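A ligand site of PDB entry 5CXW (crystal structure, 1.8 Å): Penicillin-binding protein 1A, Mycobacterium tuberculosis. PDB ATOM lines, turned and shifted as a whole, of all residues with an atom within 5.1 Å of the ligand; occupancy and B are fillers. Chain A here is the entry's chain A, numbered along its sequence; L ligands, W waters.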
ATOM      1  N   GLY A  96      26.200   4.797   5.546  1.00  0.00           N
ATOM      2  CA  GLY A  96      25.403   3.660   5.886  1.00  0.00           C
ATOM      3  C   GLY A  96      24.193   3.585   4.982  1.00  0.00           C
ATOM      4  O   GLY A  96      24.271   3.916   3.803  1.00  0.00           O
ATOM      5  N   SER A  97      23.068   3.162   5.560  1.00  0.00           N
ATOM      6  CA  SER A  97      21.866   2.840   4.794  1.00  0.00           C
ATOM      7  C   SER A  97      21.223   4.045   4.143  1.00  0.00           C
ATOM      8  O   SER A  97      20.318   3.846   3.309  1.00  0.00           O
ATOM      9  CB  SER A  97      20.842   2.178   5.663  1.00  0.00           C
ATOM     10  OG  SER A  97      21.323   0.904   6.127  1.00  0.00           O
ATOM     11  N   SER A  98      21.654   5.261   4.445  1.00  0.00           N
ATOM     12  CA  SER A  98      21.082   6.422   3.768  1.00  0.00           C
ATOM     13  C   SER A  98      21.466   6.402   2.289  1.00  0.00           C
ATOM     14  O   SER A  98      20.817   7.076   1.477  1.00  0.00           O
ATOM     15  CB  SER A  98      21.462   7.730   4.454  1.00  0.00           C
ATOM     16  OG  SER A  98      22.837   7.998   4.433  1.00  0.00           O
ATOM     17  N   LYS A 100      21.188   3.781   0.387  1.00  0.00           N
ATOM     18  CA  LYS A 100      20.375   2.827  -0.337  1.00  0.00           C
ATOM     19  C   LYS A 100      19.461   3.484  -1.384  1.00  0.00           C
ATOM     20  O   LYS A 100      19.056   2.826  -2.355  1.00  0.00           O
ATOM     21  CB  LYS A 100      19.478   1.982   0.610  1.00  0.00           C
ATOM     22  CG  LYS A 100      20.260   0.997   1.440  1.00  0.00           C
ATOM     23  CD  LYS A 100      19.413   0.250   2.435  1.00  0.00           C
ATOM     24  CE  LYS A 100      20.323  -0.634   3.244  1.00  0.00           C
ATOM     25  NZ  LYS A 100      19.604  -1.226   4.316  1.00  0.00           N
ATOM     26  N   THR A 131      24.121  -9.273   6.457  1.00  0.00           N
ATOM     27  CA  THR A 131      23.022  -9.595   7.358  1.00  0.00           C
ATOM     28  C   THR A 131      22.289  -8.299   7.687  1.00  0.00           C
ATOM     29  O   THR A 131      22.822  -7.178   7.501  1.00  0.00           O
ATOM     30  CB  THR A 131      23.451 -10.229   8.715  1.00  0.00           C
ATOM     31  OG1 THR A 131      24.360  -9.327   9.331  1.00  0.00           O
ATOM     32  CG2 THR A 131      24.231 -11.473   8.512  1.00  0.00           C
ATOM     33  N   VAL A 133      20.249  -6.007  10.695  1.00  0.00           N
ATOM     34  CA  VAL A 133      20.297  -5.754  12.159  1.00  0.00           C
ATOM     35  C   VAL A 133      19.267  -6.620  12.868  1.00  0.00           C
ATOM     36  O   VAL A 133      18.103  -6.704  12.439  1.00  0.00           O
ATOM     37  CB  VAL A 133      20.038  -4.269  12.477  1.00  0.00           C
ATOM     38  CG1 VAL A 133      19.581  -4.116  13.929  1.00  0.00           C
ATOM     39  CG2 VAL A 133      21.271  -3.438  12.209  1.00  0.00           C
ATOM     40  N   MET A 149      12.240  -0.953   5.919  1.00  0.00           N
ATOM     41  CA  MET A 149      12.806  -1.802   6.972  1.00  0.00           C
ATOM     42  C   MET A 149      14.331  -1.779   7.005  1.00  0.00           C
ATOM     43  O   MET A 149      14.965  -2.279   7.946  1.00  0.00           O
ATOM     44  CB  MET A 149      12.327  -3.244   6.792  1.00  0.00           C
ATOM     45  CG  MET A 149      10.852  -3.407   7.042  1.00  0.00           C
ATOM     46  SD  MET A 149      10.341  -5.114   6.672  1.00  0.00           S
ATOM     47  CE  MET A 149      11.188  -5.935   7.999  1.00  0.00           C
ATOM     48  N   SER A 150      14.899  -1.171   5.975  1.00  0.00           N
ATOM     49  CA  SER A 150      16.323  -1.010   5.765  1.00  0.00           C
ATOM     50  C   SER A 150      17.062  -2.337   5.785  1.00  0.00           C
ATOM     51  O   SER A 150      17.947  -2.593   6.596  1.00  0.00           O
ATOM     52  CB  SER A 150      16.920   0.021   6.706  1.00  0.00           C
ATOM     53  OG  SER A 150      18.079   0.550   6.060  1.00  0.00           O
ATOM     54  N   ASN A 152      19.617  -4.762   4.586  1.00  0.00           N
ATOM     55  CA  ASN A 152      20.914  -4.828   3.879  1.00  0.00           C
ATOM     56  C   ASN A 152      20.926  -5.939   2.836  1.00  0.00           C
ATOM     57  O   ASN A 152      21.466  -5.773   1.732  1.00  0.00           O
ATOM     58  CB  ASN A 152      22.050  -5.079   4.840  1.00  0.00           C
ATOM     59  CG  ASN A 152      22.447  -3.885   5.637  1.00  0.00           C
ATOM     60  OD1 ASN A 152      21.763  -2.846   5.692  1.00  0.00           O
ATOM     61  ND2 ASN A 152      23.609  -4.049   6.348  1.00  0.00           N
ATOM     62  N   LYS A 291      15.194   8.923   5.076  1.00  0.00           N
ATOM     63  CA  LYS A 291      15.913   7.658   5.198  1.00  0.00           C
ATOM     64  C   LYS A 291      16.982   7.798   6.289  1.00  0.00           C
ATOM     65  O   LYS A 291      17.756   8.721   6.269  1.00  0.00           O
ATOM     66  CB  LYS A 291      16.539   7.217   3.867  1.00  0.00           C
ATOM     67  CG  LYS A 291      17.208   5.834   3.971  1.00  0.00           C
ATOM     68  CD  LYS A 291      16.195   4.677   4.074  1.00  0.00           C
ATOM     69  CE  LYS A 291      16.897   3.346   4.368  1.00  0.00           C
ATOM     70  NZ  LYS A 291      17.303   3.237   5.777  1.00  0.00           N
ATOM     71  N   THR A 292      16.984   6.827   7.189  1.00  0.00           N
ATOM     72  CA  THR A 292      17.978   6.746   8.241  1.00  0.00           C
ATOM     73  C   THR A 292      19.202   5.957   7.765  1.00  0.00           C
ATOM     74  O   THR A 292      19.140   5.136   6.799  1.00  0.00           O
ATOM     75  CB  THR A 292      17.440   6.008   9.457  1.00  0.00           C
ATOM     76  OG1 THR A 292      16.863   4.771   9.037  1.00  0.00           O
ATOM     77  CG2 THR A 292      16.440   6.890  10.239  1.00  0.00           C
ATOM     78  N   GLY A 293      20.300   6.118   8.484  1.00  0.00           N
ATOM     79  CA  GLY A 293      21.477   5.255   8.325  1.00  0.00           C
ATOM     80  C   GLY A 293      22.208   5.053   9.626  1.00  0.00           C
ATOM     81  O   GLY A 293      22.228   5.959  10.425  1.00  0.00           O
ATOM     82  N   THR A 294      22.820   3.890   9.809  1.00  0.00           N
ATOM     83  CA  THR A 294      23.636   3.625  10.995  1.00  0.00           C
ATOM     84  C   THR A 294      24.791   2.723  10.552  1.00  0.00           C
ATOM     85  O   THR A 294      24.558   1.664   9.988  1.00  0.00           O
ATOM     86  CB  THR A 294      22.855   2.871  12.068  1.00  0.00           C
ATOM     87  OG1 THR A 294      21.604   3.523  12.394  1.00  0.00           O
ATOM     88  CG2 THR A 294      23.714   2.807  13.330  1.00  0.00           C
ATOM     89  N   THR A 295      26.019   3.217  10.696  1.00  0.00           N
ATOM     90  CA  THR A 295      27.230   2.428  10.341  1.00  0.00           C
ATOM     91  C   THR A 295      27.757   1.636  11.528  1.00  0.00           C
ATOM     92  O   THR A 295      27.573   1.984  12.698  1.00  0.00           O
ATOM     93  CB  THR A 295      28.326   3.297   9.761  1.00  0.00           C
ATOM     94  OG1 THR A 295      28.820   4.158  10.737  1.00  0.00           O
ATOM     95  CG2 THR A 295      27.832   4.179   8.646  1.00  0.00           C
ATOM     96  N   GLN A 296      28.462   0.555  11.184  1.00  0.00           N
ATOM     97  CA  GLN A 296      29.130  -0.281  12.153  1.00  0.00           C
ATOM     98  C   GLN A 296      30.474   0.286  12.565  1.00  0.00           C
ATOM     99  O   GLN A 296      31.263   0.751  11.739  1.00  0.00           O
ATOM    100  CB  GLN A 296      29.368  -1.671  11.522  1.00  0.00           C
ATOM    101  CG  GLN A 296      30.173  -2.638  12.357  1.00  0.00           C
ATOM    102  CD  GLN A 296      30.217  -4.004  11.681  1.00  0.00           C
ATOM    103  OE1 GLN A 296      30.177  -4.102  10.423  1.00  0.00           O
ATOM    104  NE2 GLN A 296      30.374  -5.067  12.498  1.00  0.00           N
ATOM    105  N   PHE A 297      30.764   0.163  13.867  1.00  0.00           N
ATOM    106  CA  PHE A 297      32.045   0.467  14.384  1.00  0.00           C
ATOM    107  C   PHE A 297      32.951  -0.766  14.235  1.00  0.00           C
ATOM    108  O   PHE A 297      32.695  -1.829  14.836  1.00  0.00           O
ATOM    109  CB  PHE A 297      31.993   0.910  15.858  1.00  0.00           C
ATOM    110  CG  PHE A 297      33.352   1.311  16.339  1.00  0.00           C
ATOM    111  CD1 PHE A 297      33.850   2.549  15.984  1.00  0.00           C
ATOM    112  CD2 PHE A 297      34.159   0.419  16.985  1.00  0.00           C
ATOM    113  CE1 PHE A 297      35.121   2.920  16.313  1.00  0.00           C
ATOM    114  CE2 PHE A 297      35.447   0.777  17.322  1.00  0.00           C
ATOM    115  CZ  PHE A 297      35.938   2.025  16.960  1.00  0.00           C
ATOM    116  N   THR A 300      32.775  -4.648  15.401  1.00  0.00           N
ATOM    117  CA  THR A 300      32.108  -4.784  16.697  1.00  0.00           C
ATOM    118  C   THR A 300      30.605  -4.838  16.481  1.00  0.00           C
ATOM    119  O   THR A 300      30.114  -4.745  15.370  1.00  0.00           O
ATOM    120  CB  THR A 300      32.453  -3.625  17.616  1.00  0.00           C
ATOM    121  OG1 THR A 300      31.741  -2.442  17.234  1.00  0.00           O
ATOM    122  CG2 THR A 300      33.987  -3.352  17.632  1.00  0.00           C
ATOM    123  N   THR A 301      29.863  -4.968  17.589  1.00  0.00           N
ATOM    124  CA  THR A 301      28.381  -4.920  17.516  1.00  0.00           C
ATOM    125  C   THR A 301      27.817  -3.484  17.655  1.00  0.00           C
ATOM    126  O   THR A 301      26.611  -3.284  17.643  1.00  0.00           O
ATOM    127  CB  THR A 301      27.818  -5.728  18.685  1.00  0.00           C
ATOM    128  OG1 THR A 301      28.252  -5.139  19.903  1.00  0.00           O
ATOM    129  CG2 THR A 301      28.357  -7.142  18.633  1.00  0.00           C
ATOM    130  N   ALA A 302      28.706  -2.509  17.779  1.00  0.00           N
ATOM    131  CA  ALA A 302      28.349  -1.128  18.078  1.00  0.00           C
ATOM    132  C   ALA A 302      28.387  -0.221  16.825  1.00  0.00           C
ATOM    133  O   ALA A 302      28.829  -0.648  15.744  1.00  0.00           O
ATOM    134  CB  ALA A 302      29.291  -0.628  19.164  1.00  0.00           C
ATOM    135  N   ASN A 303      27.917   1.016  16.979  1.00  0.00           N
ATOM    136  CA  ASN A 303      27.645   1.947  15.889  1.00  0.00           C
ATOM    137  C   ASN A 303      28.746   3.000  15.812  1.00  0.00           C
ATOM    138  O   ASN A 303      29.368   3.266  16.826  1.00  0.00           O
ATOM    139  CB  ASN A 303      26.292   2.643  16.094  1.00  0.00           C
ATOM    140  CG  ASN A 303      25.143   1.639  16.098  1.00  0.00           C
ATOM    141  OD1 ASN A 303      25.277   0.526  15.570  1.00  0.00           O
ATOM    142  ND2 ASN A 303      24.026   2.033  16.694  1.00  0.00           N
ATOM    143  N   TYR A 339      21.399   5.162  16.977  1.00  0.00           N
ATOM    144  CA  TYR A 339      21.064   4.838  15.579  1.00  0.00           C
ATOM    145  C   TYR A 339      20.522   6.030  14.836  1.00  0.00           C
ATOM    146  O   TYR A 339      20.169   7.039  15.421  1.00  0.00           O
ATOM    147  CB  TYR A 339      19.930   3.772  15.603  1.00  0.00           C
ATOM    148  CG  TYR A 339      20.294   2.441  16.225  1.00  0.00           C
ATOM    149  CD1 TYR A 339      20.838   1.448  15.487  1.00  0.00           C
ATOM    150  CD2 TYR A 339      20.120   2.239  17.587  1.00  0.00           C
ATOM    151  CE1 TYR A 339      21.200   0.243  16.083  1.00  0.00           C
ATOM    152  CE2 TYR A 339      20.466   1.046  18.176  1.00  0.00           C
ATOM    153  CZ  TYR A 339      20.990   0.077  17.403  1.00  0.00           C
ATOM    154  OH  TYR A 339      21.357  -1.111  17.991  1.00  0.00           O
ATOM    155  N   GLY A 340      20.402   5.941  13.520  1.00  0.00           N
ATOM    156  CA  GLY A 340      19.798   7.007  12.706  1.00  0.00           C
ATOM    157  C   GLY A 340      18.445   7.486  13.213  1.00  0.00           C
ATOM    158  O   GLY A 340      18.167   8.674  13.201  1.00  0.00           O
ATOM    159  N   SER A 341      17.651   6.544  13.717  1.00  0.00           N
ATOM    160  CA  SER A 341      16.329   6.834  14.305  1.00  0.00           C
ATOM    161  C   SER A 341      16.343   7.500  15.660  1.00  0.00           C
ATOM    162  O   SER A 341      15.258   7.820  16.184  1.00  0.00           O
ATOM    163  CB  SER A 341      15.501   5.560  14.362  1.00  0.00           C
ATOM    164  OG  SER A 341      16.160   4.648  15.254  1.00  0.00           O
HETATM  165  C1  LIG L   1      26.318  -4.162  12.002  1.00  0.00           C
HETATM  166  C2  LIG L   1      27.080  -4.434  13.139  1.00  0.00           C
HETATM  167  C3  LIG L   1      27.229  -3.474  14.117  1.00  0.00           C
HETATM  168  C4  LIG L   1      26.628  -2.240  14.002  1.00  0.00           C
HETATM  169  C5  LIG L   1      25.863  -1.943  12.897  1.00  0.00           C
HETATM  170  C6  LIG L   1      25.697  -2.924  11.882  1.00  0.00           C
HETATM  171  O1  LIG L   1      24.942  -2.705  10.759  1.00  0.00           O
HETATM  172  C7  LIG L   1      24.088  -1.570  10.717  1.00  0.00           C
HETATM  173  C8  LIG L   1      23.149  -1.716   9.543  1.00  0.00           C
HETATM  174  O2  LIG L   1      22.858  -2.822   9.117  1.00  0.00           O
HETATM  175  N1  LIG L   1      22.698  -0.565   9.074  1.00  0.00           N
HETATM  176  C9  LIG L   1      21.740  -0.516   7.973  1.00  0.00           C
HETATM  177  C10 LIG L   1      21.877   0.795   7.319  1.00  0.00           C
HETATM  178  O3  LIG L   1      22.402   1.804   7.829  1.00  0.00           O
HETATM  179  C11 LIG L   1      20.212  -0.672   8.435  1.00  0.00           C
HETATM  180  N2  LIG L   1      19.807   0.699   8.501  1.00  0.00           N
HETATM  181  S1  LIG L   1      19.864  -1.326   9.967  1.00  0.00           S
HETATM  182  C12 LIG L   1      19.295   0.120  10.745  1.00  0.00           C
HETATM  183  C13 LIG L   1      19.880   0.243  12.154  1.00  0.00           C
HETATM  184  C14 LIG L   1      17.791   0.178  10.887  1.00  0.00           C
HETATM  185  C15 LIG L   1      19.840   1.230   9.844  1.00  0.00           C
HETATM  186  C16 LIG L   1      19.192   2.579   9.858  1.00  0.00           C
HETATM  187  O4  LIG L   1      18.333   2.805   8.942  1.00  0.00           O
HETATM  188  O5  LIG L   1      19.575   3.389  10.722  1.00  0.00           O
HETATM  189  O   HOH W   1      23.590  -5.381   9.535  1.00  0.00           O
HETATM  190  O   HOH W   2      26.069  -4.889   8.649  1.00  0.00           O
HETATM  191  O   HOH W   3      25.986  -2.200   7.579  1.00  0.00           O
HETATM  192  O   HOH W   4      20.020  -4.072   8.163  1.00  0.00           O
HETATM  193  O   HOH W   5      23.837  -5.101  14.241  1.00  0.00           O
HETATM  194  O   HOH W   6      26.309  -7.746  12.537  1.00  0.00           O
HETATM  195  O   HOH W   7      17.794   3.879  12.762  1.00  0.00           O
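The backbone NH (N) of Ser 97 lies close to an oxygen (O3) of the ligand, 2.7 Å away. OG of Ser 97 is bonded to C10 of the ligand (1.3 Å). O4 of the ligand lies within hydrogen-bond range of OG1 of Thr 292 (2.5 Å). The backbone NH (N) of Thr 294 lies within hydrogen-bond range of an oxygen (O3) of the ligand, 2.9 Å away. A nitrogen (N1) of the ligand sits at hydrogen-bond distance from the backbone carbonyl oxygen of Thr 294. The side-chain hydroxyl (OG1) of Thr 294 sits at hydrogen-bond distance from an oxygen (O5) of the ligand, at 2.6 Å. The side-chain hydroxyl of Ser 150 lies within hydrogen-bond range of a nitrogen (N2) of the ligand (3.0 Å). The side-chain amide nitrogen of Asn 152 sits at hydrogen-bond distance from an oxygen (O2) of the ligand, at 3.1 Å. An oxygen (O4) of the ligand lies within salt-bridge range of the side-chain amino group (NZ) of Lys 291, 3.4 Å away.
OG of Ser 97 lies close to OG of Ser 150, 3.3 Å away. The backbone carbonyl oxygen of Thr 292 sits at hydrogen-bond distance from the backbone NH of Ser 98 (3.4 Å). OG1 of Thr 294 lies within hydrogen-bond range of N of Gly 340. The side-chain amino group (NZ) of Lys 291 lies within hydrogen-bond range of the side-chain hydroxyl (OG) of Ser 150 (2.8 Å). OG of Ser 150 is in hydrogen-bond range of NZ of Lys 100 (2.9 Å). O of Thr 131 sits at hydrogen-bond distance from ND2 of Asn 152 (3.4 Å). The backbone NH of Ala 302 lies within hydrogen-bond range of the side-chain hydroxyl of Thr 300, at 3.1 Å. The backbone carbonyl oxygen of Ala 302 lies within hydrogen-bond range of the backbone NH of Phe 297, at 2.8 Å.
Residues that only touch the ligand: Ala 302, Gly 293, Val 133, Thr 300, Gln 296, Asn 303, Thr 301, Tyr 339, Gly 96 and Gly 340. Hydrophobic or aromatic side chains within 4 Å of the ligand: Val 133 and Tyr 339. Within 4 Å of the ligand: Gly 96, Ser 97, Val 133, Ser 150, Asn 152, Lys 291, Thr 292, Gly 293, Thr 294, Gln 296, Thr 300, Thr 301, Ala 302, Asn 303, Tyr 339 and Gly 340. The nearest printed residue that does not touch the ligand is Lys 100 (4.2 Å).
Water W1 lies within hydrogen-bond range of an oxygen (O2) of the ligand, the backbone carbonyl oxygen (O) of Thr 131 and the side-chain amide nitrogen (ND2) of Asn 152. Water W7 lies within hydrogen-bond range of an oxygen (O5) of the ligand (2.8 Å), the backbone NH (N) of Ser 341 (2.8 Å) and the backbone NH (N) of Gly 340 (3.4 Å). Water W2 bridges an oxygen (O1) of the ligand (3.2 Å) and the side-chain amide nitrogen (ND2) of Asn 152 (3.5 Å). Water W3 bridges ND2 of Asn 152 (3.3 Å) and O1 of the ligand (3.4 Å).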
